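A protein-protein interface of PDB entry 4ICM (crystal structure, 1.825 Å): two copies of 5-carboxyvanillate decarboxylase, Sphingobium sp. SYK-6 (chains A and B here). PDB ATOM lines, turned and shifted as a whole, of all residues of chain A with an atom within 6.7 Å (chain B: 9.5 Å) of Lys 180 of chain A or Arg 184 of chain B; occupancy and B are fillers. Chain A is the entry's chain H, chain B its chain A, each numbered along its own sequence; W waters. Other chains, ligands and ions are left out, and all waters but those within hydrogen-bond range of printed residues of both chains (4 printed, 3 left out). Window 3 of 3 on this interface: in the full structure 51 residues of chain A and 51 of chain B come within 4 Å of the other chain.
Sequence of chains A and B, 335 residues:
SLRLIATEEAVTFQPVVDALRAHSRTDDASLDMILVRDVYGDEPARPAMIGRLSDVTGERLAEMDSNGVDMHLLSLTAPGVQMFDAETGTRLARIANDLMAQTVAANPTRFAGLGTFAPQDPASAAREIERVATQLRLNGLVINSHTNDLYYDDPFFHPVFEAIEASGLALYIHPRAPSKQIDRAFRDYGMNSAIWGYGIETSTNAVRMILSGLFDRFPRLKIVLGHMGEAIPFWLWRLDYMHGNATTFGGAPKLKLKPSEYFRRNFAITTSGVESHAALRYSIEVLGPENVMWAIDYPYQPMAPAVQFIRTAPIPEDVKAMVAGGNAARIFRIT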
ATOM      1  N   ASP A  28     -19.829  34.050   6.215  1.00  0.00           N
ATOM      2  CA  ASP A  28     -19.980  33.565   4.843  1.00  0.00           C
ATOM      3  C   ASP A  28     -20.701  32.214   4.814  1.00  0.00           C
ATOM      4  O   ASP A  28     -20.335  31.295   5.545  1.00  0.00           O
ATOM      5  CB  ASP A  28     -18.592  33.419   4.221  1.00  0.00           C
ATOM      6  CG  ASP A  28     -18.630  33.263   2.719  1.00  0.00           C
ATOM      7  OD1 ASP A  28     -19.666  32.824   2.178  1.00  0.00           O
ATOM      8  OD2 ASP A  28     -17.607  33.580   2.076  1.00  0.00           O
ATOM      9  N   ALA A  29     -21.716  32.095   3.963  1.00  0.00           N
ATOM     10  CA  ALA A  29     -22.498  30.872   3.888  1.00  0.00           C
ATOM     11  C   ALA A  29     -22.000  29.906   2.810  1.00  0.00           C
ATOM     12  O   ALA A  29     -22.528  28.810   2.677  1.00  0.00           O
ATOM     13  CB  ALA A  29     -23.967  31.199   3.674  1.00  0.00           C
ATOM     14  N   SER A  30     -20.992  30.314   2.042  1.00  0.00           N
ATOM     15  CA  SER A  30     -20.441  29.439   1.003  1.00  0.00           C
ATOM     16  C   SER A  30     -20.027  28.081   1.562  1.00  0.00           C
ATOM     17  O   SER A  30     -19.517  27.979   2.686  1.00  0.00           O
ATOM     18  CB  SER A  30     -19.254  30.099   0.280  1.00  0.00           C
ATOM     19  OG  SER A  30     -18.575  29.154  -0.543  1.00  0.00           O
ATOM     20  N   LEU A  31     -20.249  27.036   0.773  1.00  0.00           N
ATOM     21  CA  LEU A  31     -19.984  25.669   1.229  1.00  0.00           C
ATOM     22  C   LEU A  31     -18.482  25.402   1.404  1.00  0.00           C
ATOM     23  O   LEU A  31     -18.080  24.455   2.086  1.00  0.00           O
ATOM     24  CB  LEU A  31     -20.624  24.647   0.269  1.00  0.00           C
ATOM     25  CG  LEU A  31     -20.670  23.183   0.736  1.00  0.00           C
ATOM     26  CD1 LEU A  31     -21.449  23.071   2.029  1.00  0.00           C
ATOM     27  CD2 LEU A  31     -21.258  22.284  -0.354  1.00  0.00           C
ATOM     28  N   HIS A 146     -16.664  27.821  -9.629  1.00  0.00           N
ATOM     29  CA  HIS A 146     -17.498  29.036  -9.641  1.00  0.00           C
ATOM     30  C   HIS A 146     -16.850  30.249  -8.978  1.00  0.00           C
ATOM     31  O   HIS A 146     -15.954  30.126  -8.137  1.00  0.00           O
ATOM     32  CB  HIS A 146     -18.871  28.784  -8.999  1.00  0.00           C
ATOM     33  CG  HIS A 146     -18.864  28.871  -7.503  1.00  0.00           C
ATOM     34  ND1 HIS A 146     -19.057  30.057  -6.826  1.00  0.00           N
ATOM     35  CD2 HIS A 146     -18.664  27.927  -6.556  1.00  0.00           C
ATOM     36  CE1 HIS A 146     -18.997  29.835  -5.525  1.00  0.00           C
ATOM     37  NE2 HIS A 146     -18.748  28.552  -5.336  1.00  0.00           N
ATOM     38  N   ASP A 149     -20.878  32.398  -7.082  1.00  0.00           N
ATOM     39  CA  ASP A 149     -21.951  31.460  -7.388  1.00  0.00           C
ATOM     40  C   ASP A 149     -22.474  31.610  -8.817  1.00  0.00           C
ATOM     41  O   ASP A 149     -23.632  31.315  -9.109  1.00  0.00           O
ATOM     42  CB  ASP A 149     -23.060  31.528  -6.337  1.00  0.00           C
ATOM     43  CG  ASP A 149     -22.526  31.345  -4.929  1.00  0.00           C
ATOM     44  OD1 ASP A 149     -22.057  30.229  -4.610  1.00  0.00           O
ATOM     45  OD2 ASP A 149     -22.546  32.320  -4.148  1.00  0.00           O
ATOM     46  N   TYR A 151     -21.491  30.603 -12.980  1.00  0.00           N
ATOM     47  CA  TYR A 151     -20.670  29.720 -13.817  1.00  0.00           C
ATOM     48  C   TYR A 151     -20.106  30.444 -15.044  1.00  0.00           C
ATOM     49  O   TYR A 151     -20.543  31.538 -15.367  1.00  0.00           O
ATOM     50  CB  TYR A 151     -21.438  28.436 -14.179  1.00  0.00           C
ATOM     51  CG  TYR A 151     -21.753  27.628 -12.938  1.00  0.00           C
ATOM     52  CD1 TYR A 151     -20.734  26.996 -12.221  1.00  0.00           C
ATOM     53  CD2 TYR A 151     -23.049  27.541 -12.449  1.00  0.00           C
ATOM     54  CE1 TYR A 151     -21.014  26.279 -11.056  1.00  0.00           C
ATOM     55  CE2 TYR A 151     -23.337  26.827 -11.298  1.00  0.00           C
ATOM     56  CZ  TYR A 151     -22.319  26.197 -10.605  1.00  0.00           C
ATOM     57  OH  TYR A 151     -22.611  25.488  -9.449  1.00  0.00           O
ATOM     58  N   ALA A 177     -16.036  23.668  -3.615  1.00  0.00           N
ATOM     59  CA  ALA A 177     -17.295  23.094  -3.166  1.00  0.00           C
ATOM     60  C   ALA A 177     -18.456  23.614  -4.018  1.00  0.00           C
ATOM     61  O   ALA A 177     -18.390  24.731  -4.548  1.00  0.00           O
ATOM     62  CB  ALA A 177     -17.531  23.436  -1.700  1.00  0.00           C
ATOM     63  N   PRO A 178     -19.520  22.807  -4.140  1.00  0.00           N
ATOM     64  CA  PRO A 178     -20.763  23.199  -4.802  1.00  0.00           C
ATOM     65  C   PRO A 178     -21.169  24.633  -4.476  1.00  0.00           C
ATOM     66  O   PRO A 178     -21.133  25.044  -3.308  1.00  0.00           O
ATOM     67  CB  PRO A 178     -21.767  22.215  -4.210  1.00  0.00           C
ATOM     68  CG  PRO A 178     -20.971  20.965  -4.080  1.00  0.00           C
ATOM     69  CD  PRO A 178     -19.569  21.396  -3.710  1.00  0.00           C
ATOM     70  N   SER A 179     -21.542  25.385  -5.511  1.00  0.00           N
ATOM     71  CA  SER A 179     -21.959  26.777  -5.339  1.00  0.00           C
ATOM     72  C   SER A 179     -23.325  26.811  -4.687  1.00  0.00           C
ATOM     73  O   SER A 179     -23.960  25.764  -4.494  1.00  0.00           O
ATOM     74  CB  SER A 179     -22.051  27.487  -6.691  1.00  0.00           C
ATOM     75  OG  SER A 179     -23.212  27.063  -7.385  1.00  0.00           O
ATOM     76  N   LYS A 180     -23.786  28.015  -4.355  1.00  0.00           N
ATOM     77  CA  LYS A 180     -25.074  28.173  -3.690  1.00  0.00           C
ATOM     78  C   LYS A 180     -26.237  27.758  -4.585  1.00  0.00           C
ATOM     79  O   LYS A 180     -27.344  27.569  -4.095  1.00  0.00           O
ATOM     80  CB  LYS A 180     -25.270  29.605  -3.199  1.00  0.00           C
ATOM     81  CG  LYS A 180     -24.336  29.998  -2.040  1.00  0.00           C
ATOM     82  CD  LYS A 180     -24.585  31.439  -1.591  1.00  0.00           C
ATOM     83  CE  LYS A 180     -23.548  31.876  -0.555  1.00  0.00           C
ATOM     84  NZ  LYS A 180     -23.836  33.222   0.026  1.00  0.00           N
ATOM     85  N   GLN A 181     -25.996  27.618  -5.887  1.00  0.00           N
ATOM     86  CA  GLN A 181     -27.052  27.149  -6.779  1.00  0.00           C
ATOM     87  C   GLN A 181     -27.359  25.685  -6.483  1.00  0.00           C
ATOM     88  O   GLN A 181     -28.469  25.202  -6.738  1.00  0.00           O
ATOM     89  CB  GLN A 181     -26.658  27.304  -8.252  1.00  0.00           C
ATOM     90  CG  GLN A 181     -26.242  28.716  -8.669  1.00  0.00           C
ATOM     91  CD  GLN A 181     -26.291  28.896 -10.176  1.00  0.00           C
ATOM     92  OE1 GLN A 181     -27.012  28.179 -10.865  1.00  0.00           O
ATOM     93  NE2 GLN A 181     -25.526  29.857 -10.696  1.00  0.00           N
ATOM     94  N   ILE A 182     -26.373  24.972  -5.946  1.00  0.00           N
ATOM     95  CA  ILE A 182     -26.530  23.528  -5.745  1.00  0.00           C
ATOM     96  C   ILE A 182     -26.144  22.990  -4.360  1.00  0.00           C
ATOM     97  O   ILE A 182     -26.379  21.819  -4.065  1.00  0.00           O
ATOM     98  CB  ILE A 182     -25.740  22.735  -6.815  1.00  0.00           C
ATOM     99  CG1 ILE A 182     -24.260  23.131  -6.796  1.00  0.00           C
ATOM    100  CG2 ILE A 182     -26.324  22.971  -8.191  1.00  0.00           C
ATOM    101  CD1 ILE A 182     -23.391  22.169  -7.575  1.00  0.00           C
ATOM    102  N   ASP A 183     -25.569  23.830  -3.508  1.00  0.00           N
ATOM    103  CA  ASP A 183     -24.963  23.323  -2.270  1.00  0.00           C
ATOM    104  C   ASP A 183     -25.869  22.567  -1.297  1.00  0.00           C
ATOM    105  O   ASP A 183     -25.376  21.754  -0.519  1.00  0.00           O
ATOM    106  CB  ASP A 183     -24.140  24.402  -1.534  1.00  0.00           C
ATOM    107  CG  ASP A 183     -24.982  25.533  -0.982  1.00  0.00           C
ATOM    108  OD1 ASP A 183     -26.216  25.388  -0.851  1.00  0.00           O
ATOM    109  OD2 ASP A 183     -24.389  26.584  -0.667  1.00  0.00           O
ATOM    110  N   ARG A 184     -27.178  22.822  -1.349  1.00  0.00           N
ATOM    111  CA  ARG A 184     -28.138  22.210  -0.419  1.00  0.00           C
ATOM    112  C   ARG A 184     -28.068  20.676  -0.334  1.00  0.00           C
ATOM    113  O   ARG A 184     -28.281  20.100   0.731  1.00  0.00           O
ATOM    114  CB  ARG A 184     -29.568  22.655  -0.760  1.00  0.00           C
ATOM    115  CG  ARG A 184     -29.897  24.089  -0.338  1.00  0.00           C
ATOM    116  CD  ARG A 184     -31.131  24.638  -1.066  1.00  0.00           C
ATOM    117  NE  ARG A 184     -32.327  23.844  -0.795  1.00  0.00           N
ATOM    118  CZ  ARG A 184     -33.496  24.011  -1.412  1.00  0.00           C
ATOM    119  NH1 ARG A 184     -33.632  24.946  -2.345  1.00  0.00           N
ATOM    120  NH2 ARG A 184     -34.529  23.235  -1.099  1.00  0.00           N
ATOM    121  N   ARG A 187     -24.626  18.909   1.818  1.00  0.00           N
ATOM    122  CA  ARG A 187     -24.355  19.248   3.212  1.00  0.00           C
ATOM    123  C   ARG A 187     -24.137  18.022   4.105  1.00  0.00           C
ATOM    124  O   ARG A 187     -23.756  18.161   5.271  1.00  0.00           O
ATOM    125  CB  ARG A 187     -25.506  20.082   3.782  1.00  0.00           C
ATOM    126  CG  ARG A 187     -25.699  21.426   3.107  1.00  0.00           C
ATOM    127  CD  ARG A 187     -24.703  22.443   3.627  1.00  0.00           C
ATOM    128  NE  ARG A 187     -24.931  23.779   3.078  1.00  0.00           N
ATOM    129  CZ  ARG A 187     -24.235  24.854   3.430  1.00  0.00           C
ATOM    130  NH1 ARG A 187     -23.271  24.750   4.334  1.00  0.00           N
ATOM    131  NH2 ARG A 187     -24.505  26.033   2.883  1.00  0.00           N
ATOM    132  N   GLU A 201     -19.921  19.956  -9.033  1.00  0.00           N
ATOM    133  CA  GLU A 201     -19.722  21.390  -9.201  1.00  0.00           C
ATOM    134  C   GLU A 201     -18.901  21.717 -10.461  1.00  0.00           C
ATOM    135  O   GLU A 201     -19.317  22.524 -11.292  1.00  0.00           O
ATOM    136  CB  GLU A 201     -19.040  21.953  -7.942  1.00  0.00           C
ATOM    137  CG  GLU A 201     -18.288  23.252  -8.140  1.00  0.00           C
ATOM    138  CD  GLU A 201     -19.199  24.453  -8.354  1.00  0.00           C
ATOM    139  OE1 GLU A 201     -20.412  24.365  -8.065  1.00  0.00           O
ATOM    140  OE2 GLU A 201     -18.688  25.489  -8.834  1.00  0.00           O
ATOM    141  N   ARG A 208     -21.892  23.730 -18.771  1.00  0.00           N
ATOM    142  CA  ARG A 208     -22.583  24.982 -19.074  1.00  0.00           C
ATOM    143  C   ARG A 208     -21.738  25.806 -20.041  1.00  0.00           C
ATOM    144  O   ARG A 208     -22.278  26.458 -20.940  1.00  0.00           O
ATOM    145  CB  ARG A 208     -22.844  25.816 -17.814  1.00  0.00           C
ATOM    146  CG  ARG A 208     -23.826  25.221 -16.827  1.00  0.00           C
ATOM    147  CD  ARG A 208     -23.956  26.125 -15.596  1.00  0.00           C
ATOM    148  NE  ARG A 208     -24.456  27.451 -15.956  1.00  0.00           N
ATOM    149  CZ  ARG A 208     -25.712  27.862 -15.784  1.00  0.00           C
ATOM    150  NH1 ARG A 208     -26.611  27.060 -15.226  1.00  0.00           N
ATOM    151  NH2 ARG A 208     -26.068  29.086 -16.164  1.00  0.00           N
ATOM    152  N   ALA B  29     -43.466  24.810  -8.795  1.00  0.00           N
ATOM    153  CA  ALA B  29     -42.196  25.371  -9.254  1.00  0.00           C
ATOM    154  C   ALA B  29     -41.154  24.294  -9.542  1.00  0.00           C
ATOM    155  O   ALA B  29     -40.013  24.612  -9.887  1.00  0.00           O
ATOM    156  CB  ALA B  29     -41.657  26.390  -8.248  1.00  0.00           C
ATOM    157  N   SER B  30     -41.540  23.029  -9.396  1.00  0.00           N
ATOM    158  CA  SER B  30     -40.631  21.914  -9.690  1.00  0.00           C
ATOM    159  C   SER B  30     -40.055  22.027 -11.090  1.00  0.00           C
ATOM    160  O   SER B  30     -40.757  22.429 -12.020  1.00  0.00           O
ATOM    161  CB  SER B  30     -41.353  20.570  -9.572  1.00  0.00           C
ATOM    162  OG  SER B  30     -40.507  19.515 -10.021  1.00  0.00           O
ATOM    163  N   LEU B  31     -38.783  21.660 -11.239  1.00  0.00           N
ATOM    164  CA  LEU B  31     -38.113  21.718 -12.533  1.00  0.00           C
ATOM    165  C   LEU B  31     -38.744  20.755 -13.544  1.00  0.00           C
ATOM    166  O   LEU B  31     -38.620  20.950 -14.756  1.00  0.00           O
ATOM    167  CB  LEU B  31     -36.602  21.465 -12.383  1.00  0.00           C
ATOM    168  CG  LEU B  31     -35.714  21.779 -13.592  1.00  0.00           C
ATOM    169  CD1 LEU B  31     -35.824  23.245 -13.968  1.00  0.00           C
ATOM    170  CD2 LEU B  31     -34.248  21.402 -13.354  1.00  0.00           C
ATOM    171  N   ALA B 177     -36.200  15.445 -13.193  1.00  0.00           N
ATOM    172  CA  ALA B 177     -35.421  16.680 -13.258  1.00  0.00           C
ATOM    173  C   ALA B 177     -34.852  17.004 -11.867  1.00  0.00           C
ATOM    174  O   ALA B 177     -35.452  16.633 -10.861  1.00  0.00           O
ATOM    175  CB  ALA B 177     -36.273  17.826 -13.770  1.00  0.00           C
ATOM    176  N   PRO B 178     -33.685  17.673 -11.819  1.00  0.00           N
ATOM    177  CA  PRO B 178     -33.043  18.102 -10.569  1.00  0.00           C
ATOM    178  C   PRO B 178     -34.038  18.681  -9.565  1.00  0.00           C
ATOM    179  O   PRO B 178     -34.927  19.459  -9.935  1.00  0.00           O
ATOM    180  CB  PRO B 178     -32.056  19.166 -11.050  1.00  0.00           C
ATOM    181  CG  PRO B 178     -31.596  18.622 -12.382  1.00  0.00           C
ATOM    182  CD  PRO B 178     -32.853  18.000 -12.995  1.00  0.00           C
ATOM    183  N   SER B 179     -33.897  18.282  -8.305  1.00  0.00           N
ATOM    184  CA  SER B 179     -34.823  18.713  -7.270  1.00  0.00           C
ATOM    185  C   SER B 179     -34.540  20.163  -6.941  1.00  0.00           C
ATOM    186  O   SER B 179     -33.563  20.745  -7.422  1.00  0.00           O
ATOM    187  CB  SER B 179     -34.664  17.862  -6.007  1.00  0.00           C
ATOM    188  OG  SER B 179     -33.502  18.257  -5.291  1.00  0.00           O
ATOM    189  N   LYS B 180     -35.391  20.744  -6.104  1.00  0.00           N
ATOM    190  CA  LYS B 180     -35.230  22.142  -5.737  1.00  0.00           C
ATOM    191  C   LYS B 180     -33.946  22.403  -4.958  1.00  0.00           C
ATOM    192  O   LYS B 180     -33.483  23.538  -4.901  1.00  0.00           O
ATOM    193  CB  LYS B 180     -36.442  22.651  -4.962  1.00  0.00           C
ATOM    194  CG  LYS B 180     -37.698  22.814  -5.817  1.00  0.00           C
ATOM    195  CD  LYS B 180     -38.807  23.468  -5.015  1.00  0.00           C
ATOM    196  CE  LYS B 180     -40.163  23.236  -5.665  1.00  0.00           C
ATOM    197  NZ  LYS B 180     -41.265  23.771  -4.815  1.00  0.00           N
ATOM    198  N   GLN B 181     -33.354  21.362  -4.375  1.00  0.00           N
ATOM    199  CA  GLN B 181     -32.059  21.535  -3.724  1.00  0.00           C
ATOM    200  C   GLN B 181     -30.993  21.941  -4.742  1.00  0.00           C
ATOM    201  O   GLN B 181     -30.039  22.634  -4.403  1.00  0.00           O
ATOM    202  CB  GLN B 181     -31.615  20.265  -2.981  1.00  0.00           C
ATOM    203  CG  GLN B 181     -32.585  19.787  -1.910  1.00  0.00           C
ATOM    204  CD  GLN B 181     -32.009  18.670  -1.057  1.00  0.00           C
ATOM    205  OE1 GLN B 181     -30.833  18.700  -0.684  1.00  0.00           O
ATOM    206  NE2 GLN B 181     -32.836  17.671  -0.748  1.00  0.00           N
ATOM    207  N   ILE B 182     -31.148  21.508  -5.993  1.00  0.00           N
ATOM    208  CA  ILE B 182     -30.102  21.738  -6.984  1.00  0.00           C
ATOM    209  C   ILE B 182     -30.567  22.385  -8.289  1.00  0.00           C
ATOM    210  O   ILE B 182     -29.753  22.628  -9.174  1.00  0.00           O
ATOM    211  CB  ILE B 182     -29.355  20.424  -7.342  1.00  0.00           C
ATOM    212  CG1 ILE B 182     -30.318  19.378  -7.914  1.00  0.00           C
ATOM    213  CG2 ILE B 182     -28.632  19.849  -6.110  1.00  0.00           C
ATOM    214  CD1 ILE B 182     -29.604  18.216  -8.591  1.00  0.00           C
ATOM    215  N   ASP B 183     -31.856  22.675  -8.415  1.00  0.00           N
ATOM    216  CA  ASP B 183     -32.381  23.023  -9.738  1.00  0.00           C
ATOM    217  C   ASP B 183     -31.936  24.368 -10.303  1.00  0.00           C
ATOM    218  O   ASP B 183     -32.007  24.566 -11.508  1.00  0.00           O
ATOM    219  CB  ASP B 183     -33.912  22.874  -9.826  1.00  0.00           C
ATOM    220  CG  ASP B 183     -34.658  23.862  -8.953  1.00  0.00           C
ATOM    221  OD1 ASP B 183     -34.038  24.802  -8.420  1.00  0.00           O
ATOM    222  OD2 ASP B 183     -35.885  23.697  -8.809  1.00  0.00           O
ATOM    223  N   ARG B 184     -31.487  25.281  -9.441  1.00  0.00           N
ATOM    224  CA  ARG B 184     -31.081  26.611  -9.894  1.00  0.00           C
ATOM    225  C   ARG B 184     -30.057  26.564 -11.021  1.00  0.00           C
ATOM    226  O   ARG B 184     -30.084  27.405 -11.925  1.00  0.00           O
ATOM    227  CB  ARG B 184     -30.525  27.448  -8.734  1.00  0.00           C
ATOM    228  CG  ARG B 184     -31.554  28.374  -8.064  1.00  0.00           C
ATOM    229  CD  ARG B 184     -30.980  29.030  -6.794  1.00  0.00           C
ATOM    230  NE  ARG B 184     -29.798  29.850  -7.069  1.00  0.00           N
ATOM    231  CZ  ARG B 184     -29.007  30.362  -6.127  1.00  0.00           C
ATOM    232  NH1 ARG B 184     -29.270  30.138  -4.846  1.00  0.00           N
ATOM    233  NH2 ARG B 184     -27.950  31.093  -6.460  1.00  0.00           N
ATOM    234  N   ALA B 185     -29.159  25.584 -10.967  1.00  0.00           N
ATOM    235  CA  ALA B 185     -28.079  25.479 -11.950  1.00  0.00           C
ATOM    236  C   ALA B 185     -28.475  24.772 -13.249  1.00  0.00           C
ATOM    237  O   ALA B 185     -27.640  24.608 -14.151  1.00  0.00           O
ATOM    238  CB  ALA B 185     -26.883  24.782 -11.336  1.00  0.00           C
ATOM    239  N   PHE B 186     -29.733  24.345 -13.342  1.00  0.00           N
ATOM    240  CA  PHE B 186     -30.176  23.521 -14.471  1.00  0.00           C
ATOM    241  C   PHE B 186     -31.326  24.144 -15.248  1.00  0.00           C
ATOM    242  O   PHE B 186     -32.095  23.441 -15.916  1.00  0.00           O
ATOM    243  CB  PHE B 186     -30.552  22.117 -13.989  1.00  0.00           C
ATOM    244  CG  PHE B 186     -29.404  21.380 -13.354  1.00  0.00           C
ATOM    245  CD1 PHE B 186     -29.090  21.575 -12.019  1.00  0.00           C
ATOM    246  CD2 PHE B 186     -28.616  20.522 -14.103  1.00  0.00           C
ATOM    247  CE1 PHE B 186     -28.014  20.913 -11.436  1.00  0.00           C
ATOM    248  CE2 PHE B 186     -27.540  19.862 -13.530  1.00  0.00           C
ATOM    249  CZ  PHE B 186     -27.245  20.047 -12.198  1.00  0.00           C
ATOM    250  N   ARG B 187     -31.444  25.466 -15.164  1.00  0.00           N
ATOM    251  CA  ARG B 187     -32.540  26.170 -15.843  1.00  0.00           C
ATOM    252  C   ARG B 187     -32.165  26.644 -17.260  1.00  0.00           C
ATOM    253  O   ARG B 187     -33.017  27.147 -17.995  1.00  0.00           O
ATOM    254  CB  ARG B 187     -33.021  27.361 -15.000  1.00  0.00           C
ATOM    255  CG  ARG B 187     -33.683  27.001 -13.672  1.00  0.00           C
ATOM    256  CD  ARG B 187     -35.185  26.853 -13.839  1.00  0.00           C
ATOM    257  NE  ARG B 187     -35.855  26.423 -12.614  1.00  0.00           N
ATOM    258  CZ  ARG B 187     -37.141  26.089 -12.551  1.00  0.00           C
ATOM    259  NH1 ARG B 187     -37.896  26.139 -13.644  1.00  0.00           N
ATOM    260  NH2 ARG B 187     -37.676  25.701 -11.402  1.00  0.00           N
ATOM    261  N   ASP B 188     -30.902  26.481 -17.647  1.00  0.00           N
ATOM    262  CA  ASP B 188     -30.425  27.021 -18.925  1.00  0.00           C
ATOM    263  C   ASP B 188     -29.958  25.950 -19.902  1.00  0.00           C
ATOM    264  O   ASP B 188     -29.547  24.855 -19.497  1.00  0.00           O
ATOM    265  CB  ASP B 188     -29.287  28.015 -18.698  1.00  0.00           C
ATOM    266  CG  ASP B 188     -29.705  29.189 -17.846  1.00  0.00           C
ATOM    267  OD1 ASP B 188     -30.567  29.961 -18.304  1.00  0.00           O
ATOM    268  OD2 ASP B 188     -29.170  29.342 -16.722  1.00  0.00           O
ATOM    269  N   TYR B 189     -30.035  26.278 -21.190  1.00  0.00           N
ATOM    270  CA  TYR B 189     -29.491  25.451 -22.264  1.00  0.00           C
ATOM    271  C   TYR B 189     -30.083  24.046 -22.311  1.00  0.00           C
ATOM    272  O   TYR B 189     -29.424  23.116 -22.766  1.00  0.00           O
ATOM    273  CB  TYR B 189     -27.954  25.371 -22.191  1.00  0.00           C
ATOM    274  CG  TYR B 189     -27.300  26.657 -21.744  1.00  0.00           C
ATOM    275  CD1 TYR B 189     -27.480  27.832 -22.463  1.00  0.00           C
ATOM    276  CD2 TYR B 189     -26.511  26.703 -20.601  1.00  0.00           C
ATOM    277  CE1 TYR B 189     -26.894  29.013 -22.065  1.00  0.00           C
ATOM    278  CE2 TYR B 189     -25.924  27.892 -20.188  1.00  0.00           C
ATOM    279  CZ  TYR B 189     -26.124  29.041 -20.925  1.00  0.00           C
ATOM    280  OH  TYR B 189     -25.548  30.232 -20.530  1.00  0.00           O
ATOM    281  N   MET B 191     -30.636  22.040 -19.916  1.00  0.00           N
ATOM    282  CA  MET B 191     -29.969  21.131 -18.985  1.00  0.00           C
ATOM    283  C   MET B 191     -30.877  20.527 -17.904  1.00  0.00           C
ATOM    284  O   MET B 191     -30.424  19.717 -17.096  1.00  0.00           O
ATOM    285  CB  MET B 191     -28.766  21.817 -18.340  1.00  0.00           C
ATOM    286  CG  MET B 191     -27.655  22.127 -19.328  1.00  0.00           C
ATOM    287  SD  MET B 191     -26.375  23.185 -18.639  1.00  0.00           S
ATOM    288  CE  MET B 191     -25.699  22.131 -17.364  1.00  0.00           C
ATOM    289  N   ASN B 192     -32.149  20.918 -17.888  1.00  0.00           N
ATOM    290  CA  ASN B 192     -33.108  20.356 -16.936  1.00  0.00           C
ATOM    291  C   ASN B 192     -33.341  18.867 -17.182  1.00  0.00           C
ATOM    292  O   ASN B 192     -33.720  18.121 -16.276  1.00  0.00           O
ATOM    293  CB  ASN B 192     -34.446  21.100 -17.018  1.00  0.00           C
ATOM    294  CG  ASN B 192     -35.164  20.898 -18.360  1.00  0.00           C
ATOM    295  OD1 ASN B 192     -36.002  20.002 -18.507  1.00  0.00           O
ATOM    296  ND2 ASN B 192     -34.851  21.742 -19.328  1.00  0.00           N
HETATM  297  O   HOH W   1     -30.295  18.368   1.787  1.00  0.00           O
HETATM  298  O   HOH W   2     -28.354  30.041 -12.736  1.00  0.00           O
HETATM  299  O   HOH W   3     -26.111  32.139  -8.241  1.00  0.00           O
HETATM  300  O   HOH W   4     -28.749  24.821  -3.240  1.00  0.00           O
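Hydrophobic or aromatic side chains of chain B that line the printed part of chain A: Ile 182, Ala 185, Tyr 189 and Met 191. Among the printed residues, 14 pairs touch across the chains. Among the printed residues, Asp or Glu carboxylates within 4 Å of a Lys or Arg side-chain nitrogen of the other chain: Arg 208 of chain A with Asp 188 of chain B (3.2 Å).
Lys 180 of chain A touches Arg 184 of chain B, and with the chains exchanged Arg 184 of chain A touches Lys 180 of chain B. Gln 181 of chain A touches Ile 182 of chain B, and with the chains exchanged Ile 182 of chain A touches Gln 181 of chain B. Ile 182 of chain B touches its own counterpart, Ile 182 of chain A.
Water W4 lies within hydrogen-bond range of the backbone carbonyl oxygen (O) of Gln 181 of chain B (2.8 Å), the backbone NH (N) of Arg 184 of chain A (3.2 Å), the backbone carbonyl oxygen (O) of Lys 180 of chain A (3.2 Å) and the backbone NH (N) of Asp 183 of chain A (3.3 Å).
The backbone carbonyl oxygen (O) of Asp 149 of chain A sits at hydrogen-bond distance from the side-chain amide nitrogen (NE2) of Gln 181 of chain A (2.9 Å). The backbone NH of Gln 181 of chain A sits close to the side-chain hydroxyl of Ser 179 of chain A (3.2 Å).
Lys 180 of chain A touches one residue of chain B. Of the printed residues of chain A, Arg 184 of chain B touches Lys 180 (3.3 Å) and Gln 181 (3.3 Å). No residue of chain B comes within 4 Å of Ser 179 of chain A. Of chain B, only Gln 181, Ile 182, Arg 184 and Ala 185 come within 4 Å of Gln 181 of chain A. Printed residues of chain B within 4 Å of Arg 184 of chain A: Lys 180 (2.9 Å) and Gln 181 (3.2 Å). Of the printed residues of chain A, Tyr 189 of chain B touches Arg 208 (3.99 Å). The nearest residue of chain B that does not touch Lys 180 of chain A is Gln 181 of chain B (5.6 Å). The nearest residue of chain A that does not touch Arg 184 of chain B is Arg 208 of chain A (4.8 Å). The nearest printed residue of chain A that does not touch Lys 180 of chain B is Gln 181 of chain A (5.6 Å).
N of Ala 185 of chain B lies close to OE1 of Gln 181 of chain A, 3.4 Å away. The backbone carbonyl oxygen of Lys 180 of chain A sits at hydrogen-bond distance from the guanidinium group of Arg 184 of chain B. O of Arg 184 of chain B lies close to OE1 of Gln 181 of chain A (3.3 Å). The backbone carbonyl oxygen (O) of Ala 185 of chain B is in hydrogen-bond range of the guanidinium group (NH1) of Arg 208 of chain A (2.9 Å). OE1 of Gln 181 of chain B lies close to O of Arg 184 of chain A. The guanidinium group (NH2) of Arg 208 of chain A is in salt-bridge range of the side-chain carboxylate (OD2) of Asp 188 of chain B (3.2 Å). NH1 of Arg 184 of chain A sits at hydrogen-bond distance from O of Lys 180 of chain B (2.9 Å).
O of Gln 181 of chain A touches O of Ile 182 of chain B, 3.8 Å away. O of Ile 182 of chain A touches O of Gln 181 of chain B, at 3.8 Å. Ile 182 of chain A touches Ile 182 of chain B. Tyr 189 of chain B touches Arg 208 of chain A. Arg 208 of chain A touches Met 191 of chain B.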
